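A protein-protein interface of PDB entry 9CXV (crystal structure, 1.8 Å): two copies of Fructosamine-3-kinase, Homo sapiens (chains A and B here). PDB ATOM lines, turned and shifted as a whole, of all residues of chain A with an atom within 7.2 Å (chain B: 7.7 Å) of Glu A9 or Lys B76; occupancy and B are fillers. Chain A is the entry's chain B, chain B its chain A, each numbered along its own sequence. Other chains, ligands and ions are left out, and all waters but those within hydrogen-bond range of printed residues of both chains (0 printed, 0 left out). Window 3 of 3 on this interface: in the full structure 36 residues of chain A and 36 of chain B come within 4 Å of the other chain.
The backbone NH (N) of Met B75 is in hydrogen-bond range of the backbone carbonyl oxygen (O) of Val B88, at 2.8 Å. The backbone carbonyl oxygen of Lys B76 is in hydrogen-bond range of the backbone NH of Val B88. O of Ala B86 sits at hydrogen-bond distance from N of Ile B78, at 2.9 Å.
Among the printed residues, pairs that only touch across the chains: Glu A9 with Lys B76 (3.5 Å), Leu A5 with Leu B80 (3.6 Å), Glu A9 with Ile B78 (3.7 Å), Leu A5 with Ile B78 (3.7 Å), Leu A6 with Val B88 (3.8 Å) and Leu A6 with Ile B78 (3.99 Å).
Printed residues of chain B within 4 Å of Leu A5: Ile B78 and Leu B80. Printed residues of chain B within 4 Å of Leu A6: Ile B78 (3.99 Å) and Val B88 (3.8 Å). Ala A8 touches none of the printed residues of chain B. Glu A9 touches just these residues of chain B: Lys B76 (3.5 Å) and Ile B78 (3.7 Å). Phe B40 touches none of the printed residues of chain A. Of chain A, only Glu A9 comes within 4 Å of Lys B76. Of the printed residues of chain A, Leu B80 touches Leu A5 (3.6 Å). Of the printed residues of chain A, Val B88 touches Leu A6 (3.8 Å). Glu B90 touches none of the printed residues of chain A. The nearest residue of chain B that does not touch Glu A9 is Asp B79 (5.6 Å). The nearest printed residue of chain A that does not touch Leu B80 is Leu A6 (6.9 Å).
Of the 10 printed residues of chain A, 3 touch a printed residue of chain B. Hydrophobic or aromatic side chains of chain B that line the printed part of chain A: Ile B78, Leu B80 and Val B88. Among the printed residues, 6 pairs touch across the chains. Among the printed residues, no Asp or Glu carboxylate lies within 4 Å of a Lys or Arg side-chain nitrogen of the other chain.
No position is printed for both chains. Of the 6 pairs that touch across the chains among the printed residues, none has its exchanged pair printed and touching as well.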
ATOM      1  N   GLU A   3      27.591  25.272  22.801  1.00  0.00           N
ATOM      2  CA  GLU A   3      27.545  23.978  23.465  1.00  0.00           C
ATOM      3  C   GLU A   3      27.018  24.093  24.883  1.00  0.00           C
ATOM      4  O   GLU A   3      26.314  23.200  25.364  1.00  0.00           O
ATOM      5  CB  GLU A   3      28.931  23.325  23.457  1.00  0.00           C
ATOM      6  CG  GLU A   3      29.518  23.112  22.055  1.00  0.00           C
ATOM      7  CD  GLU A   3      30.315  21.789  21.888  1.00  0.00           C
ATOM      8  OE1 GLU A   3      30.499  20.990  22.856  1.00  0.00           O
ATOM      9  OE2 GLU A   3      30.733  21.540  20.741  1.00  0.00           O
ATOM     10  N   GLN A   4      27.390  25.161  25.601  1.00  0.00           N
ATOM     11  CA  GLN A   4      26.891  25.303  26.968  1.00  0.00           C
ATOM     12  C   GLN A   4      25.379  25.556  26.976  1.00  0.00           C
ATOM     13  O   GLN A   4      24.635  24.982  27.787  1.00  0.00           O
ATOM     14  CB  GLN A   4      27.665  26.426  27.655  1.00  0.00           C
ATOM     15  CG  GLN A   4      29.177  26.132  27.706  1.00  0.00           C
ATOM     16  CD  GLN A   4      29.458  24.819  28.440  1.00  0.00           C
ATOM     17  OE1 GLN A   4      28.749  24.465  29.403  1.00  0.00           O
ATOM     18  NE2 GLN A   4      30.491  24.093  27.998  1.00  0.00           N
ATOM     19  N   LEU A   5      24.934  26.415  26.064  1.00  0.00           N
ATOM     20  CA  LEU A   5      23.516  26.679  25.910  1.00  0.00           C
ATOM     21  C   LEU A   5      22.747  25.402  25.610  1.00  0.00           C
ATOM     22  O   LEU A   5      21.690  25.167  26.195  1.00  0.00           O
ATOM     23  CB  LEU A   5      23.317  27.730  24.830  1.00  0.00           C
ATOM     24  CG  LEU A   5      21.985  28.482  24.875  1.00  0.00           C
ATOM     25  CD1 LEU A   5      21.776  29.325  26.117  1.00  0.00           C
ATOM     26  CD2 LEU A   5      21.954  29.378  23.630  1.00  0.00           C
ATOM     27  N   LEU A   6      23.285  24.541  24.733  1.00  0.00           N
ATOM     28  CA  LEU A   6      22.567  23.319  24.386  1.00  0.00           C
ATOM     29  C   LEU A   6      22.535  22.374  25.573  1.00  0.00           C
ATOM     30  O   LEU A   6      21.480  21.831  25.906  1.00  0.00           O
ATOM     31  CB  LEU A   6      23.220  22.675  23.160  1.00  0.00           C
ATOM     32  CG  LEU A   6      22.909  23.437  21.883  1.00  0.00           C
ATOM     33  CD1 LEU A   6      23.771  22.985  20.677  1.00  0.00           C
ATOM     34  CD2 LEU A   6      21.397  23.339  21.535  1.00  0.00           C
ATOM     35  N   ARG A   7      23.668  22.212  26.285  1.00  0.00           N
ATOM     36  CA  ARG A   7      23.629  21.377  27.479  1.00  0.00           C
ATOM     37  C   ARG A   7      22.552  21.858  28.443  1.00  0.00           C
ATOM     38  O   ARG A   7      21.846  21.051  29.042  1.00  0.00           O
ATOM     39  CB  ARG A   7      25.005  21.356  28.179  1.00  0.00           C
ATOM     40  CG  ARG A   7      26.056  20.476  27.512  1.00  0.00           C
ATOM     41  CD  ARG A   7      27.379  20.344  28.342  1.00  0.00           C
ATOM     42  NE  ARG A   7      28.397  19.515  27.678  1.00  0.00           N
ATOM     43  CZ  ARG A   7      29.327  19.978  26.842  1.00  0.00           C
ATOM     44  NH1 ARG A   7      29.409  21.264  26.542  1.00  0.00           N
ATOM     45  NH2 ARG A   7      30.179  19.124  26.267  1.00  0.00           N
ATOM     46  N   ALA A   8      22.395  23.182  28.590  1.00  0.00           N
ATOM     47  CA  ALA A   8      21.382  23.707  29.512  1.00  0.00           C
ATOM     48  C   ALA A   8      19.949  23.587  28.965  1.00  0.00           C
ATOM     49  O   ALA A   8      19.005  23.252  29.688  1.00  0.00           O
ATOM     50  CB  ALA A   8      21.701  25.176  29.815  1.00  0.00           C
ATOM     51  N   GLU A   9      19.749  23.973  27.717  1.00  0.00           N
ATOM     52  CA  GLU A   9      18.406  23.985  27.148  1.00  0.00           C
ATOM     53  C   GLU A   9      17.840  22.581  27.028  1.00  0.00           C
ATOM     54  O   GLU A   9      16.627  22.385  27.200  1.00  0.00           O
ATOM     55  CB  GLU A   9      18.439  24.644  25.774  1.00  0.00           C
ATOM     56  CG  GLU A   9      18.744  26.119  25.805  1.00  0.00           C
ATOM     57  CD  GLU A   9      17.549  26.963  26.203  1.00  0.00           C
ATOM     58  OE1 GLU A   9      16.415  26.422  26.252  1.00  0.00           O
ATOM     59  OE2 GLU A   9      17.761  28.164  26.479  1.00  0.00           O
ATOM     60  N   LEU A  10      18.696  21.607  26.694  1.00  0.00           N
ATOM     61  CA  LEU A  10      18.302  20.202  26.544  1.00  0.00           C
ATOM     62  C   LEU A  10      18.564  19.360  27.782  1.00  0.00           C
ATOM     63  O   LEU A  10      18.135  18.202  27.813  1.00  0.00           O
ATOM     64  CB  LEU A  10      19.041  19.535  25.373  1.00  0.00           C
ATOM     65  CG  LEU A  10      18.959  20.190  23.996  1.00  0.00           C
ATOM     66  CD1 LEU A  10      19.796  19.406  22.954  1.00  0.00           C
ATOM     67  CD2 LEU A  10      17.503  20.406  23.578  1.00  0.00           C
ATOM     68  N   ARG A  11      19.275  19.890  28.784  1.00  0.00           N
ATOM     69  CA  ARG A  11      19.507  19.188  30.052  1.00  0.00           C
ATOM     70  C   ARG A  11      20.246  17.863  29.833  1.00  0.00           C
ATOM     71  O   ARG A  11      19.804  16.797  30.241  1.00  0.00           O
ATOM     72  CB  ARG A  11      18.181  18.975  30.797  1.00  0.00           C
ATOM     73  CG  ARG A  11      17.181  20.110  30.593  1.00  0.00           C
ATOM     74  CD  ARG A  11      16.365  20.426  31.832  1.00  0.00           C
ATOM     75  NE  ARG A  11      15.044  20.966  31.501  1.00  0.00           N
ATOM     76  CZ  ARG A  11      14.594  22.168  31.857  1.00  0.00           C
ATOM     77  NH1 ARG A  11      15.355  23.031  32.517  1.00  0.00           N
ATOM     78  NH2 ARG A  11      13.348  22.515  31.545  1.00  0.00           N
ATOM     79  N   THR A  12      21.412  17.953  29.209  1.00  0.00           N
ATOM     80  CA  THR A  12      22.235  16.782  28.939  1.00  0.00           C
ATOM     81  C   THR A  12      23.629  17.031  29.507  1.00  0.00           C
ATOM     82  O   THR A  12      24.124  18.165  29.473  1.00  0.00           O
ATOM     83  CB  THR A  12      22.304  16.463  27.392  1.00  0.00           C
ATOM     84  OG1 THR A  12      23.353  15.521  27.101  1.00  0.00           O
ATOM     85  CG2 THR A  12      22.590  17.726  26.569  1.00  0.00           C
ATOM     86  N   PHE B  40      19.831  17.065  16.031  1.00  0.00           N
ATOM     87  CA  PHE B  40      20.371  17.867  14.971  1.00  0.00           C
ATOM     88  C   PHE B  40      19.989  19.311  15.233  1.00  0.00           C
ATOM     89  O   PHE B  40      18.823  19.609  15.514  1.00  0.00           O
ATOM     90  CB  PHE B  40      19.887  17.371  13.593  1.00  0.00           C
ATOM     91  CG  PHE B  40      20.528  18.093  12.472  1.00  0.00           C
ATOM     92  CD1 PHE B  40      21.751  17.664  11.974  1.00  0.00           C
ATOM     93  CD2 PHE B  40      19.949  19.226  11.937  1.00  0.00           C
ATOM     94  CE1 PHE B  40      22.372  18.360  10.948  1.00  0.00           C
ATOM     95  CE2 PHE B  40      20.551  19.916  10.910  1.00  0.00           C
ATOM     96  CZ  PHE B  40      21.771  19.490  10.406  1.00  0.00           C
ATOM     97  N   VAL B  41      20.973  20.207  15.177  1.00  0.00           N
ATOM     98  CA  VAL B  41      20.780  21.600  15.556  1.00  0.00           C
ATOM     99  C   VAL B  41      21.076  22.472  14.365  1.00  0.00           C
ATOM    100  O   VAL B  41      22.159  22.377  13.771  1.00  0.00           O
ATOM    101  CB  VAL B  41      21.666  22.002  16.767  1.00  0.00           C
ATOM    102  CG1 VAL B  41      21.412  23.436  17.108  1.00  0.00           C
ATOM    103  CG2 VAL B  41      21.343  21.120  17.927  1.00  0.00           C
ATOM    104  N   LYS B  42      20.104  23.308  14.007  1.00  0.00           N
ATOM    105  CA  LYS B  42      20.234  24.297  12.951  1.00  0.00           C
ATOM    106  C   LYS B  42      20.482  25.628  13.602  1.00  0.00           C
ATOM    107  O   LYS B  42      19.763  26.012  14.519  1.00  0.00           O
ATOM    108  CB  LYS B  42      18.965  24.442  12.089  1.00  0.00           C
ATOM    109  CG  LYS B  42      18.717  23.393  11.014  1.00  0.00           C
ATOM    110  CD  LYS B  42      17.585  23.913  10.064  1.00  0.00           C
ATOM    111  CE  LYS B  42      16.997  22.765   9.320  1.00  0.00           C
ATOM    112  NZ  LYS B  42      16.059  23.220   8.241  1.00  0.00           N
ATOM    113  N   ARG B  50      14.145  33.444  14.432  1.00  0.00           N
ATOM    114  CA  ARG B  50      13.093  32.804  15.226  1.00  0.00           C
ATOM    115  C   ARG B  50      11.810  32.650  14.415  1.00  0.00           C
ATOM    116  O   ARG B  50      11.187  31.587  14.437  1.00  0.00           O
ATOM    117  CB  ARG B  50      12.799  33.581  16.520  1.00  0.00           C
ATOM    118  CG  ARG B  50      11.563  33.009  17.251  1.00  0.00           C
ATOM    119  CD  ARG B  50      11.348  33.515  18.672  1.00  0.00           C
ATOM    120  NE  ARG B  50      12.111  32.759  19.646  1.00  0.00           N
ATOM    121  CZ  ARG B  50      11.730  31.593  20.159  1.00  0.00           C
ATOM    122  NH1 ARG B  50      10.613  30.998  19.780  1.00  0.00           N
ATOM    123  NH2 ARG B  50      12.498  31.001  21.061  1.00  0.00           N
ATOM    124  N   PHE B  53      12.267  29.837  11.982  1.00  0.00           N
ATOM    125  CA  PHE B  53      12.206  28.513  12.556  1.00  0.00           C
ATOM    126  C   PHE B  53      10.803  28.207  13.035  1.00  0.00           C
ATOM    127  O   PHE B  53      10.393  27.043  13.034  1.00  0.00           O
ATOM    128  CB  PHE B  53      13.210  28.399  13.701  1.00  0.00           C
ATOM    129  CG  PHE B  53      14.654  28.240  13.216  1.00  0.00           C
ATOM    130  CD1 PHE B  53      14.959  27.405  12.132  1.00  0.00           C
ATOM    131  CD2 PHE B  53      15.700  28.927  13.846  1.00  0.00           C
ATOM    132  CE1 PHE B  53      16.279  27.247  11.688  1.00  0.00           C
ATOM    133  CE2 PHE B  53      17.025  28.772  13.410  1.00  0.00           C
ATOM    134  CZ  PHE B  53      17.321  27.927  12.339  1.00  0.00           C
ATOM    135  N   VAL B  57       8.808  24.877  12.211  1.00  0.00           N
ATOM    136  CA  VAL B  57       8.147  24.053  13.222  1.00  0.00           C
ATOM    137  C   VAL B  57       6.682  23.880  12.868  1.00  0.00           C
ATOM    138  O   VAL B  57       6.154  22.767  12.944  1.00  0.00           O
ATOM    139  CB  VAL B  57       8.269  24.681  14.615  1.00  0.00           C
ATOM    140  CG1 VAL B  57       7.235  23.985  15.591  1.00  0.00           C
ATOM    141  CG2 VAL B  57       9.739  24.582  15.119  1.00  0.00           C
ATOM    142  N   ARG B  73      11.165  15.345  14.230  1.00  0.00           N
ATOM    143  CA  ARG B  73      10.298  15.922  15.244  1.00  0.00           C
ATOM    144  C   ARG B  73      10.946  17.186  15.774  1.00  0.00           C
ATOM    145  O   ARG B  73      12.090  17.125  16.245  1.00  0.00           O
ATOM    146  CB  ARG B  73      10.069  14.927  16.397  1.00  0.00           C
ATOM    147  CG  ARG B  73       9.018  15.453  17.427  1.00  0.00           C
ATOM    148  CD  ARG B  73       8.729  14.508  18.590  1.00  0.00           C
ATOM    149  NE  ARG B  73       9.936  14.267  19.375  1.00  0.00           N
ATOM    150  CZ  ARG B  73      10.270  14.914  20.487  1.00  0.00           C
ATOM    151  NH1 ARG B  73       9.475  15.832  21.026  1.00  0.00           N
ATOM    152  NH2 ARG B  73      11.435  14.639  21.069  1.00  0.00           N
ATOM    153  N   PRO B  74      10.286  18.335  15.701  1.00  0.00           N
ATOM    154  CA  PRO B  74      10.866  19.552  16.292  1.00  0.00           C
ATOM    155  C   PRO B  74      10.942  19.431  17.808  1.00  0.00           C
ATOM    156  O   PRO B  74      10.050  18.882  18.453  1.00  0.00           O
ATOM    157  CB  PRO B  74       9.889  20.663  15.863  1.00  0.00           C
ATOM    158  CG  PRO B  74       8.644  19.957  15.420  1.00  0.00           C
ATOM    159  CD  PRO B  74       9.016  18.596  14.996  1.00  0.00           C
ATOM    160  N   MET B  75      12.015  19.956  18.377  1.00  0.00           N
ATOM    161  CA  MET B  75      12.219  19.900  19.827  1.00  0.00           C
ATOM    162  C   MET B  75      12.204  21.276  20.471  1.00  0.00           C
ATOM    163  O   MET B  75      11.417  21.521  21.388  1.00  0.00           O
ATOM    164  CB  MET B  75      13.545  19.215  20.097  1.00  0.00           C
ATOM    165  CG  MET B  75      13.372  17.694  19.930  1.00  0.00           C
ATOM    166  SD  MET B  75      14.974  16.884  19.882  1.00  0.00           S
ATOM    167  CE  MET B  75      15.436  16.917  21.629  1.00  0.00           C
ATOM    168  N   LYS B  76      13.012  22.207  19.981  1.00  0.00           N
ATOM    169  CA  LYS B  76      13.107  23.457  20.723  1.00  0.00           C
ATOM    170  C   LYS B  76      13.597  24.558  19.806  1.00  0.00           C
ATOM    171  O   LYS B  76      14.489  24.318  18.986  1.00  0.00           O
ATOM    172  CB  LYS B  76      14.095  23.316  21.924  1.00  0.00           C
ATOM    173  CG  LYS B  76      13.749  24.218  23.131  1.00  0.00           C
ATOM    174  CD  LYS B  76      14.391  23.691  24.438  1.00  0.00           C
ATOM    175  CE  LYS B  76      13.695  24.279  25.678  1.00  0.00           C
ATOM    176  NZ  LYS B  76      12.438  23.538  26.047  1.00  0.00           N
ATOM    177  N   VAL B  77      13.051  25.771  19.964  1.00  0.00           N
ATOM    178  CA  VAL B  77      13.629  26.949  19.324  1.00  0.00           C
ATOM    179  C   VAL B  77      14.222  27.840  20.429  1.00  0.00           C
ATOM    180  O   VAL B  77      13.495  28.268  21.336  1.00  0.00           O
ATOM    181  CB  VAL B  77      12.604  27.725  18.481  1.00  0.00           C
ATOM    182  CG1 VAL B  77      13.267  29.020  17.949  1.00  0.00           C
ATOM    183  CG2 VAL B  77      12.050  26.820  17.302  1.00  0.00           C
ATOM    184  N   ILE B  78      15.510  28.163  20.310  1.00  0.00           N
ATOM    185  CA  ILE B  78      16.299  28.823  21.354  1.00  0.00           C
ATOM    186  C   ILE B  78      16.752  30.190  20.829  1.00  0.00           C
ATOM    187  O   ILE B  78      17.375  30.277  19.763  1.00  0.00           O
ATOM    188  CB  ILE B  78      17.525  27.966  21.731  1.00  0.00           C
ATOM    189  CG1 ILE B  78      17.074  26.622  22.268  1.00  0.00           C
ATOM    190  CG2 ILE B  78      18.381  28.666  22.782  1.00  0.00           C
ATOM    191  CD1 ILE B  78      18.143  25.542  22.208  1.00  0.00           C
ATOM    192  N   ASP B  79      16.468  31.248  21.585  1.00  0.00           N
ATOM    193  CA  ASP B  79      17.005  32.559  21.237  1.00  0.00           C
ATOM    194  C   ASP B  79      18.479  32.597  21.611  1.00  0.00           C
ATOM    195  O   ASP B  79      18.857  32.229  22.730  1.00  0.00           O
ATOM    196  CB  ASP B  79      16.240  33.667  21.947  1.00  0.00           C
ATOM    197  CG  ASP B  79      14.771  33.660  21.603  1.00  0.00           C
ATOM    198  OD1 ASP B  79      14.424  33.981  20.434  1.00  0.00           O
ATOM    199  OD2 ASP B  79      13.963  33.303  22.503  1.00  0.00           O
ATOM    200  N   LEU B  80      19.344  33.003  20.621  1.00  0.00           N
ATOM    201  CA  LEU B  80      20.796  32.949  20.803  1.00  0.00           C
ATOM    202  C   LEU B  80      21.309  34.291  21.322  1.00  0.00           C
ATOM    203  O   LEU B  80      20.896  35.343  20.818  1.00  0.00           O
ATOM    204  CB  LEU B  80      21.498  32.586  19.498  1.00  0.00           C
ATOM    205  CG  LEU B  80      21.352  31.120  19.044  1.00  0.00           C
ATOM    206  CD1 LEU B  80      22.150  30.850  17.794  1.00  0.00           C
ATOM    207  CD2 LEU B  80      21.754  30.107  20.132  1.00  0.00           C
ATOM    208  N   ALA B  85      18.874  32.346  16.307  1.00  0.00           N
ATOM    209  CA  ALA B  85      18.249  31.268  17.053  1.00  0.00           C
ATOM    210  C   ALA B  85      18.826  29.932  16.597  1.00  0.00           C
ATOM    211  O   ALA B  85      19.397  29.794  15.504  1.00  0.00           O
ATOM    212  CB  ALA B  85      16.709  31.359  16.914  1.00  0.00           C
ATOM    213  N   ALA B  86      18.730  28.966  17.485  1.00  0.00           N
ATOM    214  CA  ALA B  86      19.008  27.583  17.168  1.00  0.00           C
ATOM    215  C   ALA B  86      17.673  26.839  17.149  1.00  0.00           C
ATOM    216  O   ALA B  86      16.727  27.198  17.863  1.00  0.00           O
ATOM    217  CB  ALA B  86      19.971  26.970  18.157  1.00  0.00           C
ATOM    218  N   PHE B  87      17.579  25.840  16.280  1.00  0.00           N
ATOM    219  CA  PHE B  87      16.395  24.989  16.204  1.00  0.00           C
ATOM    220  C   PHE B  87      16.890  23.572  16.364  1.00  0.00           C
ATOM    221  O   PHE B  87      17.712  23.101  15.570  1.00  0.00           O
ATOM    222  CB  PHE B  87      15.653  25.224  14.862  1.00  0.00           C
ATOM    223  CG  PHE B  87      14.546  24.244  14.591  1.00  0.00           C
ATOM    224  CD1 PHE B  87      13.803  23.708  15.634  1.00  0.00           C
ATOM    225  CD2 PHE B  87      14.272  23.838  13.272  1.00  0.00           C
ATOM    226  CE1 PHE B  87      12.782  22.770  15.378  1.00  0.00           C
ATOM    227  CE2 PHE B  87      13.252  22.906  12.982  1.00  0.00           C
ATOM    228  CZ  PHE B  87      12.506  22.366  14.027  1.00  0.00           C
ATOM    229  N   VAL B  88      16.472  22.933  17.438  1.00  0.00           N
ATOM    230  CA  VAL B  88      16.890  21.587  17.774  1.00  0.00           C
ATOM    231  C   VAL B  88      15.776  20.626  17.356  1.00  0.00           C
ATOM    232  O   VAL B  88      14.594  20.857  17.689  1.00  0.00           O
ATOM    233  CB  VAL B  88      17.158  21.468  19.273  1.00  0.00           C
ATOM    234  CG1 VAL B  88      17.726  20.115  19.542  1.00  0.00           C
ATOM    235  CG2 VAL B  88      18.113  22.619  19.706  1.00  0.00           C
ATOM    236  N   MET B  89      16.149  19.541  16.658  1.00  0.00           N
ATOM    237  CA  MET B  89      15.137  18.571  16.259  1.00  0.00           C
ATOM    238  C   MET B  89      15.718  17.162  16.431  1.00  0.00           C
ATOM    239  O   MET B  89      16.936  16.980  16.545  1.00  0.00           O
ATOM    240  CB  MET B  89      14.697  18.696  14.786  1.00  0.00           C
ATOM    241  CG  MET B  89      15.754  18.397  13.749  1.00  0.00           C
ATOM    242  SD  MET B  89      15.277  19.057  12.165  1.00  0.00           S
ATOM    243  CE  MET B  89      15.779  20.774  12.255  1.00  0.00           C
ATOM    244  N   GLU B  90      14.827  16.170  16.482  1.00  0.00           N
ATOM    245  CA  GLU B  90      15.225  14.762  16.442  1.00  0.00           C
ATOM    246  C   GLU B  90      16.228  14.516  15.316  1.00  0.00           C
ATOM    247  O   GLU B  90      16.090  15.033  14.204  1.00  0.00           O
ATOM    248  CB  GLU B  90      13.978  13.899  16.233  1.00  0.00           C
ATOM    249  CG  GLU B  90      14.191  12.397  15.935  1.00  0.00           C
ATOM    250  CD  GLU B  90      12.946  11.795  15.322  1.00  0.00           C
ATOM    251  OE1 GLU B  90      12.188  12.559  14.651  1.00  0.00           O
ATOM    252  OE2 GLU B  90      12.684  10.598  15.562  1.00  0.00           O
